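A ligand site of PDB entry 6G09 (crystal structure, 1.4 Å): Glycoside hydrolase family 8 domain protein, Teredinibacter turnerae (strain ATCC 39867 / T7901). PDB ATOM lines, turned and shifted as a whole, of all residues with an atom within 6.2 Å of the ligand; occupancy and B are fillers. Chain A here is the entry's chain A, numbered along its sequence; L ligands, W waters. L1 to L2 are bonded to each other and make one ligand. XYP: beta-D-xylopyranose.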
ATOM      1  N   GLU A  73      12.626   9.574  -5.018  1.00  0.00           N
ATOM      2  CA  GLU A  73      11.472  10.349  -4.510  1.00  0.00           C
ATOM      3  C   GLU A  73      11.949  11.755  -4.214  1.00  0.00           C
ATOM      4  O   GLU A  73      11.300  12.747  -4.598  1.00  0.00           O
ATOM      5  CB  GLU A  73      10.858   9.736  -3.249  1.00  0.00           C
ATOM      6  CG  GLU A  73      10.033   8.523  -3.545  1.00  0.00           C
ATOM      7  CD  GLU A  73       9.405   7.915  -2.308  1.00  0.00           C
ATOM      8  OE1 GLU A  73       9.705   8.332  -1.165  1.00  0.00           O
ATOM      9  OE2 GLU A  73       8.625   6.945  -2.475  1.00  0.00           O
ATOM     10  N   TRP A 117      15.798   3.742  -7.169  1.00  0.00           N
ATOM     11  CA  TRP A 117      15.159   4.480  -6.068  1.00  0.00           C
ATOM     12  C   TRP A 117      16.188   4.979  -5.055  1.00  0.00           C
ATOM     13  O   TRP A 117      15.920   5.925  -4.316  1.00  0.00           O
ATOM     14  CB  TRP A 117      14.088   3.650  -5.375  1.00  0.00           C
ATOM     15  CG  TRP A 117      14.518   2.584  -4.428  1.00  0.00           C
ATOM     16  CD1 TRP A 117      14.781   1.272  -4.733  1.00  0.00           C
ATOM     17  CD2 TRP A 117      14.715   2.715  -3.018  1.00  0.00           C
ATOM     18  NE1 TRP A 117      15.156   0.596  -3.592  1.00  0.00           N
ATOM     19  CE2 TRP A 117      15.158   1.462  -2.535  1.00  0.00           C
ATOM     20  CE3 TRP A 117      14.650   3.790  -2.116  1.00  0.00           C
ATOM     21  CZ2 TRP A 117      15.455   1.238  -1.188  1.00  0.00           C
ATOM     22  CZ3 TRP A 117      14.891   3.546  -0.775  1.00  0.00           C
ATOM     23  CH2 TRP A 117      15.314   2.285  -0.332  1.00  0.00           C
ATOM     24  N   ASP A 127      19.994   0.025  -5.470  1.00  0.00           N
ATOM     25  CA  ASP A 127      18.915  -0.808  -6.041  1.00  0.00           C
ATOM     26  C   ASP A 127      18.552  -0.135  -7.356  1.00  0.00           C
ATOM     27  O   ASP A 127      18.167   1.046  -7.310  1.00  0.00           O
ATOM     28  CB  ASP A 127      17.738  -0.902  -5.072  1.00  0.00           C
ATOM     29  CG  ASP A 127      16.586  -1.802  -5.460  1.00  0.00           C
ATOM     30  OD1 ASP A 127      16.608  -2.317  -6.583  1.00  0.00           O
ATOM     31  OD2 ASP A 127      15.705  -1.998  -4.599  1.00  0.00           O
ATOM     32  N   MET A 129      15.940  -0.908  -9.125  1.00  0.00           N
ATOM     33  CA  MET A 129      14.476  -0.865  -9.221  1.00  0.00           C
ATOM     34  C   MET A 129      13.973   0.492  -8.736  1.00  0.00           C
ATOM     35  O   MET A 129      14.590   1.151  -7.884  1.00  0.00           O
ATOM     36  CB  MET A 129      13.835  -1.954  -8.392  1.00  0.00           C
ATOM     37  CG  MET A 129      14.114  -3.378  -8.889  1.00  0.00           C
ATOM     38  SD  MET A 129      13.227  -3.675 -10.468  1.00  0.00           S
ATOM     39  CE  MET A 129      14.618  -3.911 -11.533  1.00  0.00           C
ATOM     40  N   PRO A 130      12.809   0.946  -9.249  1.00  0.00           N
ATOM     41  CA  PRO A 130      12.297   2.244  -8.863  1.00  0.00           C
ATOM     42  C   PRO A 130      11.365   2.239  -7.656  1.00  0.00           C
ATOM     43  O   PRO A 130      10.925   1.174  -7.217  1.00  0.00           O
ATOM     44  CB  PRO A 130      11.466   2.661 -10.070  1.00  0.00           C
ATOM     45  CG  PRO A 130      10.929   1.311 -10.577  1.00  0.00           C
ATOM     46  CD  PRO A 130      12.084   0.371 -10.385  1.00  0.00           C
ATOM     47  N   ALA A 131      11.129   3.417  -7.123  1.00  0.00           N
ATOM     48  CA  ALA A 131      10.010   3.715  -6.205  1.00  0.00           C
ATOM     49  C   ALA A 131       9.006   4.485  -7.027  1.00  0.00           C
ATOM     50  O   ALA A 131       9.232   5.667  -7.326  1.00  0.00           O
ATOM     51  CB  ALA A 131      10.414   4.491  -4.982  1.00  0.00           C
ATOM     52  N   PRO A 132       7.917   3.857  -7.513  1.00  0.00           N
ATOM     53  CA  PRO A 132       7.139   4.472  -8.581  1.00  0.00           C
ATOM     54  C   PRO A 132       6.521   5.856  -8.340  1.00  0.00           C
ATOM     55  O   PRO A 132       6.302   6.567  -9.305  1.00  0.00           O
ATOM     56  CB  PRO A 132       6.045   3.430  -8.844  1.00  0.00           C
ATOM     57  CG  PRO A 132       6.772   2.139  -8.562  1.00  0.00           C
ATOM     58  CD  PRO A 132       7.568   2.435  -7.323  1.00  0.00           C
ATOM     59  N   ASP A 133       6.323   6.287  -7.127  1.00  0.00           N
ATOM     60  CA  ASP A 133       5.884   7.668  -6.938  1.00  0.00           C
ATOM     61  C   ASP A 133       6.955   8.673  -7.334  1.00  0.00           C
ATOM     62  O   ASP A 133       6.577   9.808  -7.740  1.00  0.00           O
ATOM     63  CB  ASP A 133       5.361   7.941  -5.535  1.00  0.00           C
ATOM     64  CG  ASP A 133       6.423   7.867  -4.439  1.00  0.00           C
ATOM     65  OD1 ASP A 133       7.287   6.981  -4.533  1.00  0.00           O
ATOM     66  OD2 ASP A 133       6.323   8.721  -3.518  1.00  0.00           O
ATOM     67  N   ARG A 181      21.835  -6.345  -8.199  1.00  0.00           N
ATOM     68  CA  ARG A 181      21.410  -7.308  -7.149  1.00  0.00           C
ATOM     69  C   ARG A 181      21.401  -8.744  -7.718  1.00  0.00           C
ATOM     70  O   ARG A 181      20.967  -9.622  -6.984  1.00  0.00           O
ATOM     71  CB  ARG A 181      20.040  -6.864  -6.595  1.00  0.00           C
ATOM     72  CG  ARG A 181      20.041  -5.596  -5.761  1.00  0.00           C
ATOM     73  CD  ARG A 181      18.660  -4.930  -5.622  1.00  0.00           C
ATOM     74  NE  ARG A 181      17.722  -5.860  -5.002  1.00  0.00           N
ATOM     75  CZ  ARG A 181      16.396  -5.856  -5.178  1.00  0.00           C
ATOM     76  NH1 ARG A 181      15.784  -4.989  -5.985  1.00  0.00           N
ATOM     77  NH2 ARG A 181      15.689  -6.763  -4.519  1.00  0.00           N
ATOM     78  N   MET A 184      17.120 -10.124 -12.290  1.00  0.00           N
ATOM     79  CA  MET A 184      15.770  -9.730 -11.841  1.00  0.00           C
ATOM     80  C   MET A 184      14.837  -9.629 -13.045  1.00  0.00           C
ATOM     81  O   MET A 184      15.297  -9.522 -14.218  1.00  0.00           O
ATOM     82  CB  MET A 184      15.819  -8.383 -11.099  1.00  0.00           C
ATOM     83  CG  MET A 184      16.820  -8.388  -9.937  1.00  0.00           C
ATOM     84  SD  MET A 184      16.504  -7.111  -8.672  1.00  0.00           S
ATOM     85  CE  MET A 184      16.861  -5.675  -9.676  1.00  0.00           C
ATOM     86  N   PHE A 199       3.426  -0.823  -6.235  1.00  0.00           N
ATOM     87  CA  PHE A 199       4.488  -0.600  -5.254  1.00  0.00           C
ATOM     88  C   PHE A 199       5.859  -0.828  -5.909  1.00  0.00           C
ATOM     89  O   PHE A 199       6.822  -0.098  -5.610  1.00  0.00           O
ATOM     90  CB  PHE A 199       4.274  -1.502  -4.028  1.00  0.00           C
ATOM     91  CG  PHE A 199       5.436  -1.473  -3.090  1.00  0.00           C
ATOM     92  CD1 PHE A 199       5.663  -0.324  -2.336  1.00  0.00           C
ATOM     93  CD2 PHE A 199       6.387  -2.492  -3.064  1.00  0.00           C
ATOM     94  CE1 PHE A 199       6.775  -0.219  -1.493  1.00  0.00           C
ATOM     95  CE2 PHE A 199       7.485  -2.410  -2.202  1.00  0.00           C
ATOM     96  CZ  PHE A 199       7.691  -1.253  -1.485  1.00  0.00           C
ATOM     97  N   THR A 200       5.977  -1.876  -6.719  1.00  0.00           N
ATOM     98  CA  THR A 200       7.240  -2.193  -7.416  1.00  0.00           C
ATOM     99  C   THR A 200       6.934  -2.869  -8.738  1.00  0.00           C
ATOM    100  O   THR A 200       5.965  -3.602  -8.811  1.00  0.00           O
ATOM    101  CB  THR A 200       8.130  -3.143  -6.587  1.00  0.00           C
ATOM    102  OG1 THR A 200       9.373  -3.328  -7.267  1.00  0.00           O
ATOM    103  CG2 THR A 200       7.527  -4.485  -6.284  1.00  0.00           C
ATOM    104  N   ASP A 202       9.041  -5.061  -9.792  1.00  0.00           N
ATOM    105  CA  ASP A 202       9.714  -6.370  -9.609  1.00  0.00           C
ATOM    106  C   ASP A 202       8.629  -7.439  -9.625  1.00  0.00           C
ATOM    107  O   ASP A 202       7.719  -7.381  -8.806  1.00  0.00           O
ATOM    108  CB  ASP A 202      10.514  -6.377  -8.307  1.00  0.00           C
ATOM    109  CG  ASP A 202      11.161  -7.697  -7.921  1.00  0.00           C
ATOM    110  OD1 ASP A 202      10.927  -8.716  -8.600  1.00  0.00           O
ATOM    111  OD2 ASP A 202      11.847  -7.732  -6.835  1.00  0.00           O
ATOM    112  N   ASN A 204       8.433 -10.283  -8.469  1.00  0.00           N
ATOM    113  CA  ASN A 204       8.248 -11.019  -7.189  1.00  0.00           C
ATOM    114  C   ASN A 204       7.180 -10.352  -6.332  1.00  0.00           C
ATOM    115  O   ASN A 204       6.676 -11.010  -5.417  1.00  0.00           O
ATOM    116  CB  ASN A 204       9.566 -11.234  -6.460  1.00  0.00           C
ATOM    117  CG  ASN A 204      10.445 -12.261  -7.150  1.00  0.00           C
ATOM    118  OD1 ASN A 204       9.931 -13.162  -7.825  1.00  0.00           O
ATOM    119  ND2 ASN A 204      11.729 -12.016  -7.069  1.00  0.00           N
ATOM    120  N   ASN A 205       6.924  -9.056  -6.507  1.00  0.00           N
ATOM    121  CA  ASN A 205       5.996  -8.357  -5.614  1.00  0.00           C
ATOM    122  C   ASN A 205       5.174  -7.344  -6.418  1.00  0.00           C
ATOM    123  O   ASN A 205       4.711  -6.370  -5.827  1.00  0.00           O
ATOM    124  CB  ASN A 205       6.730  -7.649  -4.462  1.00  0.00           C
ATOM    125  CG  ASN A 205       7.313  -8.640  -3.476  1.00  0.00           C
ATOM    126  OD1 ASN A 205       6.566  -9.278  -2.733  1.00  0.00           O
ATOM    127  ND2 ASN A 205       8.628  -8.669  -3.391  1.00  0.00           N
ATOM    128  N   TYR A 213       1.102   6.406  -3.096  1.00  0.00           N
ATOM    129  CA  TYR A 213       1.567   6.551  -4.487  1.00  0.00           C
ATOM    130  C   TYR A 213       0.404   6.933  -5.405  1.00  0.00           C
ATOM    131  O   TYR A 213       0.621   7.283  -6.568  1.00  0.00           O
ATOM    132  CB  TYR A 213       2.196   5.262  -4.986  1.00  0.00           C
ATOM    133  CG  TYR A 213       3.496   4.832  -4.354  1.00  0.00           C
ATOM    134  CD1 TYR A 213       4.065   5.456  -3.251  1.00  0.00           C
ATOM    135  CD2 TYR A 213       4.153   3.728  -4.870  1.00  0.00           C
ATOM    136  CE1 TYR A 213       5.278   5.007  -2.748  1.00  0.00           C
ATOM    137  CE2 TYR A 213       5.338   3.242  -4.318  1.00  0.00           C
ATOM    138  CZ  TYR A 213       5.914   3.899  -3.253  1.00  0.00           C
ATOM    139  OH  TYR A 213       7.091   3.449  -2.704  1.00  0.00           O
ATOM    140  N   TYR A 259       1.396   0.062   2.698  1.00  0.00           N
ATOM    141  CA  TYR A 259       1.297  -0.742   1.470  1.00  0.00           C
ATOM    142  C   TYR A 259      -0.056  -1.439   1.399  1.00  0.00           C
ATOM    143  O   TYR A 259      -0.690  -1.714   2.426  1.00  0.00           O
ATOM    144  CB  TYR A 259       2.366  -1.833   1.378  1.00  0.00           C
ATOM    145  CG  TYR A 259       3.805  -1.433   1.531  1.00  0.00           C
ATOM    146  CD1 TYR A 259       4.214  -0.105   1.369  1.00  0.00           C
ATOM    147  CD2 TYR A 259       4.803  -2.373   1.771  1.00  0.00           C
ATOM    148  CE1 TYR A 259       5.531   0.291   1.565  1.00  0.00           C
ATOM    149  CE2 TYR A 259       6.129  -1.989   1.969  1.00  0.00           C
ATOM    150  CZ  TYR A 259       6.478  -0.672   1.887  1.00  0.00           C
ATOM    151  OH  TYR A 259       7.797  -0.323   2.105  1.00  0.00           O
ATOM    152  N   TRP A 267      -1.550  -4.583   2.809  1.00  0.00           N
ATOM    153  CA  TRP A 267      -0.635  -5.664   2.410  1.00  0.00           C
ATOM    154  C   TRP A 267       0.570  -5.648   3.363  1.00  0.00           C
ATOM    155  O   TRP A 267       1.205  -4.577   3.527  1.00  0.00           O
ATOM    156  CB  TRP A 267      -0.203  -5.523   0.954  1.00  0.00           C
ATOM    157  CG  TRP A 267       0.931  -6.423   0.563  1.00  0.00           C
ATOM    158  CD1 TRP A 267       1.038  -7.764   0.795  1.00  0.00           C
ATOM    159  CD2 TRP A 267       2.151  -6.012  -0.052  1.00  0.00           C
ATOM    160  NE1 TRP A 267       2.229  -8.217   0.340  1.00  0.00           N
ATOM    161  CE2 TRP A 267       2.915  -7.196  -0.232  1.00  0.00           C
ATOM    162  CE3 TRP A 267       2.582  -4.822  -0.607  1.00  0.00           C
ATOM    163  CZ2 TRP A 267       4.216  -7.137  -0.782  1.00  0.00           C
ATOM    164  CZ3 TRP A 267       3.829  -4.785  -1.198  1.00  0.00           C
ATOM    165  CH2 TRP A 267       4.603  -5.935  -1.276  1.00  0.00           C
ATOM    166  N   TRP A 271       9.148  -8.755   4.000  1.00  0.00           N
ATOM    167  CA  TRP A 271      10.376  -8.145   4.585  1.00  0.00           C
ATOM    168  C   TRP A 271      10.009  -7.002   5.541  1.00  0.00           C
ATOM    169  O   TRP A 271      10.904  -6.404   6.164  1.00  0.00           O
ATOM    170  CB  TRP A 271      11.295  -7.669   3.468  1.00  0.00           C
ATOM    171  CG  TRP A 271      10.755  -6.496   2.739  1.00  0.00           C
ATOM    172  CD1 TRP A 271      11.018  -5.194   3.010  1.00  0.00           C
ATOM    173  CD2 TRP A 271       9.860  -6.513   1.611  1.00  0.00           C
ATOM    174  NE1 TRP A 271      10.332  -4.386   2.165  1.00  0.00           N
ATOM    175  CE2 TRP A 271       9.628  -5.168   1.293  1.00  0.00           C
ATOM    176  CE3 TRP A 271       9.253  -7.532   0.862  1.00  0.00           C
ATOM    177  CZ2 TRP A 271       8.721  -4.800   0.308  1.00  0.00           C
ATOM    178  CZ3 TRP A 271       8.426  -7.145  -0.180  1.00  0.00           C
ATOM    179  CH2 TRP A 271       8.192  -5.803  -0.439  1.00  0.00           C
ATOM    180  N   ASP A 281       5.136   6.205   4.846  1.00  0.00           N
ATOM    181  CA  ASP A 281       4.543   6.389   3.517  1.00  0.00           C
ATOM    182  C   ASP A 281       3.177   7.033   3.675  1.00  0.00           C
ATOM    183  O   ASP A 281       2.859   7.973   2.917  1.00  0.00           O
ATOM    184  CB  ASP A 281       4.358   5.066   2.775  1.00  0.00           C
ATOM    185  CG  ASP A 281       5.594   4.457   2.168  1.00  0.00           C
ATOM    186  OD1 ASP A 281       6.658   4.440   2.870  1.00  0.00           O
ATOM    187  OD2 ASP A 281       5.539   3.904   1.063  1.00  0.00           O
HETATM  188  O1  XYP L   1      10.545   2.972  -1.316  1.00  0.00           O
HETATM  189  C1  XYP L   1      11.293   1.804  -1.707  1.00  0.00           C
HETATM  190  C2  XYP L   1      11.117   0.775  -0.631  1.00  0.00           C
HETATM  191  C3  XYP L   1      11.917  -0.438  -1.045  1.00  0.00           C
HETATM  192  C4  XYP L   1      11.468  -0.856  -2.401  1.00  0.00           C
HETATM  193  C5  XYP L   1      11.568   0.268  -3.413  1.00  0.00           C
HETATM  194  O2  XYP L   1      11.609   1.282   0.614  1.00  0.00           O
HETATM  195  O3  XYP L   1      11.696  -1.485  -0.096  1.00  0.00           O
HETATM  196  O4  XYP L   1      12.343  -1.931  -2.901  1.00  0.00           O
HETATM  197  O5  XYP L   1      10.778   1.367  -2.947  1.00  0.00           O
HETATM  198  C1  XYP L   2      11.642  -2.958  -3.582  1.00  0.00           C
HETATM  199  C2  XYP L   2      12.705  -3.713  -4.372  1.00  0.00           C
HETATM  200  C3  XYP L   2      12.011  -4.883  -5.080  1.00  0.00           C
HETATM  201  C4  XYP L   2      11.268  -5.692  -4.031  1.00  0.00           C
HETATM  202  C5  XYP L   2      10.315  -4.811  -3.249  1.00  0.00           C
HETATM  203  O2  XYP L   2      13.240  -2.872  -5.396  1.00  0.00           O
HETATM  204  O3  XYP L   2      13.027  -5.643  -5.738  1.00  0.00           O
HETATM  205  O4  XYP L   2      10.462  -6.699  -4.763  1.00  0.00           O
HETATM  206  O5  XYP L   2      11.061  -3.822  -2.644  1.00  0.00           O
HETATM  207  O   HOH W   1      13.765  -3.340  -0.249  1.00  0.00           O
HETATM  208  O   HOH W   2       8.299   1.678  -4.098  1.00  0.00           O
HETATM  209  O   HOH W   3      11.494   5.519  -1.940  1.00  0.00           O
HETATM  210  O   HOH W   4      13.626   0.464   2.226  1.00  0.00           O
HETATM  211  O   HOH W   5      10.197  -1.534   2.176  1.00  0.00           O
HETATM  212  O   HOH W   6      11.074  -1.426  -6.549  1.00  0.00           O
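An oxygen (O3) of XYP L2 is in hydrogen-bond range of the side-chain carboxylate (OD2) of Asp 202 (2.6 Å). OD2 of Asp 127 lies within hydrogen-bond range of O2 of XYP L2 (2.7 Å). The guanidinium group (NH1) of Arg 181 lies within hydrogen-bond range of an oxygen (O3) of XYP L2 (2.8 Å). The side-chain amide nitrogen (ND2) of Asn 205 lies within hydrogen-bond range of an oxygen (O4) of XYP L2 (3.0 Å).
N of Asp 202 sits at hydrogen-bond distance from OG1 of Thr 200, 3.1 Å away. OD1 of Asp 202 is in hydrogen-bond range of N of Asn 204. NH1 of Arg 181 is in salt-bridge range of OD1 of Asp 127, at 2.9 Å. N of Met 129 is in hydrogen-bond range of OD1 of Asp 127 (3.0 Å). NE1 of Trp 117 is in hydrogen-bond range of OD2 of Asp 127 (2.8 Å). The guanidinium group (NH1) of Arg 181 lies within hydrogen-bond range of the side-chain sulfur (SD) of Met 184 (3.5 Å). The backbone carbonyl oxygen (O) of Met 129 is in hydrogen-bond range of the backbone NH (N) of Trp 117, 2.9 Å away.
Merely in contact with the ligand: Trp 117, Met 129, Pro 130, Ala 131, Phe 199, Thr 200, Tyr 213 and Trp 271. Hydrophobic or aromatic side chains within 4 Å of the ligand: Trp 117, Met 129, Ala 131, Phe 199 and Trp 271. Of the 20 residues printed, 12 come within 4 Å of the ligand. The nearest printed residue that does not touch the ligand is Tyr 259 (4.4 Å).
Water W5 lies within hydrogen-bond range of the side-chain hydroxyl of Tyr 259 (2.7 Å), an oxygen (O3) of XYP L1 (2.7 Å) and the indole nitrogen of Trp 271 (2.9 Å). Water W2 lies within hydrogen-bond range of the side-chain hydroxyl (OH) of Tyr 213 (2.6 Å), an oxygen (O5) of XYP L1 (2.8 Å) and the backbone carbonyl oxygen (O) of Phe 199 (2.8 Å). Water W3 bridges an oxygen (O1) of XYP L1 (2.8 Å) and the side-chain carboxylate of Glu 73 (3.2 Å). Water W6 lies within hydrogen-bond range of the side-chain hydroxyl of Thr 200 (2.7 Å), the backbone carbonyl oxygen of Pro 130 (2.7 Å) and an oxygen (O2) of XYP L2 (2.8 Å).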
